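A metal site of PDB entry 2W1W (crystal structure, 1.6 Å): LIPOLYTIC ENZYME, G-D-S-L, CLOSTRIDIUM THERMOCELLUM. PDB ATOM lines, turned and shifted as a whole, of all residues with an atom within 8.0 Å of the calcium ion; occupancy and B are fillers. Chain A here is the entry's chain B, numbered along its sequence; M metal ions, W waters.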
ATOM      1  N   ILE A   6      30.142   9.227  -3.805  1.00  0.00           N
ATOM      2  CA  ILE A   6      28.697   9.331  -3.537  1.00  0.00           C
ATOM      3  C   ILE A   6      28.184   8.109  -2.811  1.00  0.00           C
ATOM      4  O   ILE A   6      28.310   6.969  -3.281  1.00  0.00           O
ATOM      5  CB  ILE A   6      27.894   9.500  -4.845  1.00  0.00           C
ATOM      6  CG1 ILE A   6      28.425  10.664  -5.631  1.00  0.00           C
ATOM      7  CG2 ILE A   6      26.381   9.592  -4.540  1.00  0.00           C
ATOM      8  CD1 ILE A   6      28.470  11.880  -4.963  1.00  0.00           C
ATOM      9  N   TYR A   7      27.583   8.381  -1.664  1.00  0.00           N
ATOM     10  CA  TYR A   7      26.947   7.378  -0.785  1.00  0.00           C
ATOM     11  C   TYR A   7      25.429   7.548  -0.985  1.00  0.00           C
ATOM     12  O   TYR A   7      24.825   8.416  -0.415  1.00  0.00           O
ATOM     13  CB  TYR A   7      27.447   7.593   0.661  1.00  0.00           C
ATOM     14  CG  TYR A   7      28.916   7.308   0.799  1.00  0.00           C
ATOM     15  CD1 TYR A   7      29.381   6.025   1.012  1.00  0.00           C
ATOM     16  CD2 TYR A   7      29.854   8.305   0.656  1.00  0.00           C
ATOM     17  CE1 TYR A   7      30.715   5.755   1.087  1.00  0.00           C
ATOM     18  CE2 TYR A   7      31.210   8.037   0.742  1.00  0.00           C
ATOM     19  CZ  TYR A   7      31.633   6.754   0.955  1.00  0.00           C
ATOM     20  OH  TYR A   7      32.978   6.456   1.034  1.00  0.00           O
ATOM     21  N   GLN A   8      24.882   6.727  -1.861  1.00  0.00           N
ATOM     22  CA  GLN A   8      23.464   6.794  -2.227  1.00  0.00           C
ATOM     23  C   GLN A   8      22.590   6.309  -1.073  1.00  0.00           C
ATOM     24  O   GLN A   8      22.984   5.501  -0.258  1.00  0.00           O
ATOM     25  CB  GLN A   8      23.156   5.975  -3.496  1.00  0.00           C
ATOM     26  CG  GLN A   8      23.542   6.717  -4.763  1.00  0.00           C
ATOM     27  CD  GLN A   8      22.648   7.927  -5.068  1.00  0.00           C
ATOM     28  OE1 GLN A   8      22.938   8.677  -6.009  1.00  0.00           O
ATOM     29  NE2 GLN A   8      21.563   8.069  -4.354  1.00  0.00           N
ATOM     30  N   ALA A   9      21.376   6.821  -1.068  1.00  0.00           N
ATOM     31  CA  ALA A   9      20.339   6.394  -0.118  1.00  0.00           C
ATOM     32  C   ALA A   9      20.245   4.863  -0.010  1.00  0.00           C
ATOM     33  O   ALA A   9      20.063   4.305   1.070  1.00  0.00           O
ATOM     34  CB  ALA A   9      19.016   7.019  -0.513  1.00  0.00           C
ATOM     35  N   GLU A  10      20.352   4.181  -1.150  1.00  0.00           N
ATOM     36  CA  GLU A  10      20.118   2.739  -1.198  1.00  0.00           C
ATOM     37  C   GLU A  10      21.179   1.971  -0.422  1.00  0.00           C
ATOM     38  O   GLU A  10      20.977   0.832   0.028  1.00  0.00           O
ATOM     39  CB  GLU A  10      19.979   2.252  -2.656  1.00  0.00           C
ATOM     40  CG  GLU A  10      21.201   2.008  -3.431  1.00  0.00           C
ATOM     41  CD  GLU A  10      20.854   1.404  -4.832  1.00  0.00           C
ATOM     42  OE1 GLU A  10      19.793   0.732  -4.950  1.00  0.00           O
ATOM     43  OE2 GLU A  10      21.609   1.638  -5.782  1.00  0.00           O
ATOM     44  N   ASP A  11      22.306   2.626  -0.216  1.00  0.00           N
ATOM     45  CA  ASP A  11      23.453   2.023   0.470  1.00  0.00           C
ATOM     46  C   ASP A  11      23.553   2.356   1.971  1.00  0.00           C
ATOM     47  O   ASP A  11      24.429   1.828   2.685  1.00  0.00           O
ATOM     48  CB  ASP A  11      24.732   2.396  -0.217  1.00  0.00           C
ATOM     49  CG  ASP A  11      24.931   1.625  -1.529  1.00  0.00           C
ATOM     50  OD1 ASP A  11      24.508   0.460  -1.645  1.00  0.00           O
ATOM     51  OD2 ASP A  11      25.403   2.223  -2.489  1.00  0.00           O
ATOM     52  N   LEU A  19      12.949   3.963   2.212  1.00  0.00           N
ATOM     53  CA  LEU A  19      13.361   4.319   0.843  1.00  0.00           C
ATOM     54  C   LEU A  19      12.122   4.472  -0.001  1.00  0.00           C
ATOM     55  O   LEU A  19      11.160   3.689   0.104  1.00  0.00           O
ATOM     56  CB  LEU A  19      14.264   3.252   0.231  1.00  0.00           C
ATOM     57  CG  LEU A  19      15.515   2.900   1.052  1.00  0.00           C
ATOM     58  CD1 LEU A  19      16.289   1.703   0.420  1.00  0.00           C
ATOM     59  CD2 LEU A  19      16.417   4.124   1.267  1.00  0.00           C
ATOM     60  N   GLU A  20      12.128   5.502  -0.810  1.00  0.00           N
ATOM     61  CA  GLU A  20      11.005   5.753  -1.708  1.00  0.00           C
ATOM     62  C   GLU A  20      11.419   6.562  -2.916  1.00  0.00           C
ATOM     63  O   GLU A  20      12.542   7.055  -3.029  1.00  0.00           O
ATOM     64  CB  GLU A  20       9.824   6.430  -0.977  1.00  0.00           C
ATOM     65  CG  GLU A  20      10.071   7.829  -0.610  1.00  0.00           C
ATOM     66  CD  GLU A  20       8.856   8.537   0.073  1.00  0.00           C
ATOM     67  OE1 GLU A  20       8.117   7.846   0.783  1.00  0.00           O
ATOM     68  OE2 GLU A  20       8.664   9.775  -0.132  1.00  0.00           O
ATOM     69  N   GLY A  25      13.253  13.975  -8.805  1.00  0.00           N
ATOM     70  CA  GLY A  25      14.514  14.753  -8.811  1.00  0.00           C
ATOM     71  C   GLY A  25      15.659  14.182  -7.984  1.00  0.00           C
ATOM     72  O   GLY A  25      16.756  14.718  -7.920  1.00  0.00           O
ATOM     73  N   TYR A  26      15.358  13.038  -7.378  1.00  0.00           N
ATOM     74  CA  TYR A  26      16.370  12.220  -6.694  1.00  0.00           C
ATOM     75  C   TYR A  26      17.294  11.645  -7.767  1.00  0.00           C
ATOM     76  O   TYR A  26      17.024  11.693  -8.974  1.00  0.00           O
ATOM     77  CB  TYR A  26      15.765  11.106  -5.817  1.00  0.00           C
ATOM     78  CG  TYR A  26      14.937  10.112  -6.601  1.00  0.00           C
ATOM     79  CD1 TYR A  26      15.510   8.976  -7.142  1.00  0.00           C
ATOM     80  CD2 TYR A  26      13.601  10.343  -6.861  1.00  0.00           C
ATOM     81  CE1 TYR A  26      14.771   8.084  -7.874  1.00  0.00           C
ATOM     82  CE2 TYR A  26      12.841   9.453  -7.582  1.00  0.00           C
ATOM     83  CZ  TYR A  26      13.434   8.342  -8.120  1.00  0.00           C
ATOM     84  OH  TYR A  26      12.665   7.481  -8.891  1.00  0.00           O
ATOM     85  N   THR A  27      18.391  11.121  -7.276  1.00  0.00           N
ATOM     86  CA  THR A  27      19.371  10.376  -8.085  1.00  0.00           C
ATOM     87  C   THR A  27      19.533   8.962  -7.593  1.00  0.00           C
ATOM     88  O   THR A  27      19.100   8.580  -6.500  1.00  0.00           O
ATOM     89  CB  THR A  27      20.733  11.051  -8.143  1.00  0.00           C
ATOM     90  OG1 THR A  27      21.309  11.101  -6.831  1.00  0.00           O
ATOM     91  CG2 THR A  27      20.616  12.483  -8.761  1.00  0.00           C
ATOM     92  N   GLY A  28      20.152   8.140  -8.441  1.00  0.00           N
ATOM     93  CA  GLY A  28      20.186   6.708  -8.143  1.00  0.00           C
ATOM     94  C   GLY A  28      18.786   6.095  -8.106  1.00  0.00           C
ATOM     95  O   GLY A  28      17.888   6.530  -8.770  1.00  0.00           O
ATOM     96  N   SER A  29      18.639   5.088  -7.287  1.00  0.00           N
ATOM     97  CA  SER A  29      17.397   4.299  -7.282  1.00  0.00           C
ATOM     98  C   SER A  29      16.279   4.822  -6.404  1.00  0.00           C
ATOM     99  O   SER A  29      15.155   4.357  -6.482  1.00  0.00           O
ATOM    100  CB  SER A  29      17.698   2.860  -6.867  1.00  0.00           C
ATOM    101  OG  SER A  29      18.143   2.746  -5.521  1.00  0.00           O
ATOM    102  N   CYS A  30      16.618   5.757  -5.531  1.00  0.00           N
ATOM    103  CA  CYS A  30      15.701   6.196  -4.472  1.00  0.00           C
ATOM    104  C   CYS A  30      16.303   7.290  -3.592  1.00  0.00           C
ATOM    105  O   CYS A  30      17.457   7.664  -3.743  1.00  0.00           O
ATOM    106  CB  CYS A  30      15.305   5.026  -3.589  1.00  0.00           C
ATOM    107  SG  CYS A  30      16.681   4.317  -2.648  1.00  0.00           S
ATOM    108  N   TYR A  31      15.462   7.757  -2.686  1.00  0.00           N
ATOM    109  CA  TYR A  31      15.889   8.663  -1.567  1.00  0.00           C
ATOM    110  C   TYR A  31      15.306   8.129  -0.278  1.00  0.00           C
ATOM    111  O   TYR A  31      14.463   7.266  -0.290  1.00  0.00           O
ATOM    112  CB  TYR A  31      15.490  10.121  -1.825  1.00  0.00           C
ATOM    113  CG  TYR A  31      14.012  10.324  -1.929  1.00  0.00           C
ATOM    114  CD1 TYR A  31      13.227  10.524  -0.780  1.00  0.00           C
ATOM    115  CD2 TYR A  31      13.369  10.328  -3.166  1.00  0.00           C
ATOM    116  CE1 TYR A  31      11.894  10.722  -0.861  1.00  0.00           C
ATOM    117  CE2 TYR A  31      12.026  10.500  -3.232  1.00  0.00           C
ATOM    118  CZ  TYR A  31      11.283  10.709  -2.093  1.00  0.00           C
ATOM    119  OH  TYR A  31       9.925  10.864  -2.165  1.00  0.00           O
ATOM    120  N   VAL A  32      15.761   8.681   0.843  1.00  0.00           N
ATOM    121  CA  VAL A  32      15.241   8.342   2.170  1.00  0.00           C
ATOM    122  C   VAL A  32      14.237   9.377   2.651  1.00  0.00           C
ATOM    123  O   VAL A  32      14.478  10.583   2.596  1.00  0.00           O
ATOM    124  CB  VAL A  32      16.359   8.302   3.225  1.00  0.00           C
ATOM    125  CG1 VAL A  32      15.781   7.886   4.589  1.00  0.00           C
ATOM    126  CG2 VAL A  32      17.463   7.372   2.790  1.00  0.00           C
ATOM    127  N   TRP A  44      25.972   5.662   6.963  1.00  0.00           N
ATOM    128  CA  TRP A  44      26.763   5.024   5.899  1.00  0.00           C
ATOM    129  C   TRP A  44      28.140   4.661   6.400  1.00  0.00           C
ATOM    130  O   TRP A  44      28.730   5.310   7.296  1.00  0.00           O
ATOM    131  CB  TRP A  44      27.007   5.987   4.750  1.00  0.00           C
ATOM    132  CG  TRP A  44      25.852   6.281   3.861  1.00  0.00           C
ATOM    133  CD1 TRP A  44      25.449   5.575   2.756  1.00  0.00           C
ATOM    134  CD2 TRP A  44      25.015   7.444   3.909  1.00  0.00           C
ATOM    135  NE1 TRP A  44      24.413   6.210   2.127  1.00  0.00           N
ATOM    136  CE2 TRP A  44      24.114   7.352   2.805  1.00  0.00           C
ATOM    137  CE3 TRP A  44      24.877   8.541   4.792  1.00  0.00           C
ATOM    138  CZ2 TRP A  44      23.156   8.319   2.559  1.00  0.00           C
ATOM    139  CZ3 TRP A  44      23.959   9.488   4.501  1.00  0.00           C
ATOM    140  CH2 TRP A  44      23.102   9.373   3.405  1.00  0.00           C
ATOM    141  N   ARG A  59      22.781  15.984  -0.238  1.00  0.00           N
ATOM    142  CA  ARG A  59      21.745  16.457  -1.178  1.00  0.00           C
ATOM    143  C   ARG A  59      20.400  16.031  -0.631  1.00  0.00           C
ATOM    144  O   ARG A  59      20.183  14.847  -0.313  1.00  0.00           O
ATOM    145  CB  ARG A  59      21.979  15.923  -2.592  1.00  0.00           C
ATOM    146  CG  ARG A  59      21.021  16.492  -3.645  1.00  0.00           C
ATOM    147  CD  ARG A  59      21.441  16.034  -5.040  1.00  0.00           C
ATOM    148  NE  ARG A  59      20.734  16.740  -6.104  1.00  0.00           N
ATOM    149  CZ  ARG A  59      19.613  16.303  -6.684  1.00  0.00           C
ATOM    150  NH1 ARG A  59      19.102  15.160  -6.340  1.00  0.00           N
ATOM    151  NH2 ARG A  59      18.994  17.020  -7.635  1.00  0.00           N
ATOM    152  N   TRP A  94      15.878  19.986  -4.765  1.00  0.00           N
ATOM    153  CA  TRP A  94      16.997  19.372  -4.043  1.00  0.00           C
ATOM    154  C   TRP A  94      18.205  20.301  -3.973  1.00  0.00           C
ATOM    155  O   TRP A  94      18.708  20.790  -4.982  1.00  0.00           O
ATOM    156  CB  TRP A  94      17.400  18.021  -4.669  1.00  0.00           C
ATOM    157  CG  TRP A  94      16.273  17.064  -4.820  1.00  0.00           C
ATOM    158  CD1 TRP A  94      15.324  17.049  -5.800  1.00  0.00           C
ATOM    159  CD2 TRP A  94      15.945  15.960  -3.944  1.00  0.00           C
ATOM    160  NE1 TRP A  94      14.437  16.024  -5.608  1.00  0.00           N
ATOM    161  CE2 TRP A  94      14.784  15.350  -4.459  1.00  0.00           C
ATOM    162  CE3 TRP A  94      16.515  15.448  -2.767  1.00  0.00           C
ATOM    163  CZ2 TRP A  94      14.202  14.233  -3.858  1.00  0.00           C
ATOM    164  CZ3 TRP A  94      15.922  14.359  -2.169  1.00  0.00           C
ATOM    165  CH2 TRP A  94      14.774  13.762  -2.701  1.00  0.00           C
ATOM    166  N   VAL A 123      16.430  12.754   1.987  1.00  0.00           N
ATOM    167  CA  VAL A 123      17.874  12.759   1.683  1.00  0.00           C
ATOM    168  C   VAL A 123      18.169  11.844   0.490  1.00  0.00           C
ATOM    169  O   VAL A 123      17.839  10.663   0.481  1.00  0.00           O
ATOM    170  CB  VAL A 123      18.753  12.342   2.905  1.00  0.00           C
ATOM    171  CG1 VAL A 123      20.229  12.293   2.488  1.00  0.00           C
ATOM    172  CG2 VAL A 123      18.490  13.285   4.095  1.00  0.00           C
ATOM    173  N   ASP A 124      18.777  12.449  -0.521  1.00  0.00           N
ATOM    174  CA  ASP A 124      19.142  11.772  -1.778  1.00  0.00           C
ATOM    175  C   ASP A 124      20.417  10.944  -1.637  1.00  0.00           C
ATOM    176  O   ASP A 124      20.468   9.750  -2.013  1.00  0.00           O
ATOM    177  CB  ASP A 124      19.266  12.796  -2.903  1.00  0.00           C
ATOM    178  CG  ASP A 124      19.411  12.166  -4.288  1.00  0.00           C
ATOM    179  OD1 ASP A 124      18.901  11.040  -4.502  1.00  0.00           O
ATOM    180  OD2 ASP A 124      20.065  12.816  -5.138  1.00  0.00           O
ATOM    181  N   TYR A 125      21.436  11.585  -1.077  1.00  0.00           N
ATOM    182  CA  TYR A 125      22.756  11.003  -0.917  1.00  0.00           C
ATOM    183  C   TYR A 125      23.630  11.850   0.001  1.00  0.00           C
ATOM    184  O   TYR A 125      23.289  12.992   0.313  1.00  0.00           O
ATOM    185  CB  TYR A 125      23.454  10.760  -2.274  1.00  0.00           C
ATOM    186  CG  TYR A 125      23.817  11.999  -3.088  1.00  0.00           C
ATOM    187  CD1 TYR A 125      24.736  12.949  -2.643  1.00  0.00           C
ATOM    188  CD2 TYR A 125      23.288  12.154  -4.352  1.00  0.00           C
ATOM    189  CE1 TYR A 125      25.059  14.052  -3.435  1.00  0.00           C
ATOM    190  CE2 TYR A 125      23.614  13.207  -5.150  1.00  0.00           C
ATOM    191  CZ  TYR A 125      24.524  14.150  -4.711  1.00  0.00           C
ATOM    192  OH  TYR A 125      24.842  15.253  -5.513  1.00  0.00           O
ATOM    193  N   LEU A 126      24.731  11.241   0.437  1.00  0.00           N
ATOM    194  CA  LEU A 126      25.882  11.925   1.055  1.00  0.00           C
ATOM    195  C   LEU A 126      27.064  11.804   0.095  1.00  0.00           C
ATOM    196  O   LEU A 126      27.401  10.711  -0.371  1.00  0.00           O
ATOM    197  CB  LEU A 126      26.221  11.300   2.405  1.00  0.00           C
ATOM    198  CG  LEU A 126      27.533  11.703   3.049  1.00  0.00           C
ATOM    199  CD1 LEU A 126      27.484  13.186   3.368  1.00  0.00           C
ATOM    200  CD2 LEU A 126      27.844  10.863   4.306  1.00  0.00           C
HETATM  201 CA    CA M   1      19.435   8.785  -4.189  1.00  0.00          CA
HETATM  202  O   HOH W   1      19.746   5.421  -3.766  1.00  0.00           O
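NE1 of Trp 44 sits at hydrogen-bond distance from O of Gln 8 (2.9 Å). The side-chain sulfur (SG) of Cys 30 sits at hydrogen-bond distance from the side-chain hydroxyl (OG) of Ser 29 (3.6 Å). O of Asp 124 lies close to N of Ala 9 (3.2 Å). The guanidinium group of Arg 59 lies within salt-bridge range of the side-chain carboxylate of Asp 124 (2.8 Å).
Water W1 lies within hydrogen-bond range of the backbone NH of Glu 10 (3.0 Å), the side-chain sulfur of Cys 30 (3.4 Å) and the backbone NH of Ala 9 (3.4 Å).
The calcium ion is bound by NE2 of Gln 8 (2.3 Å), O of Cys 30 (2.3 Å), OD1 of Asp 124 (2.3 Å), O of Thr 27 (2.3 Å) and O of Asp 124 (2.6 Å). The calcium ion has five donor atoms within binding distance.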
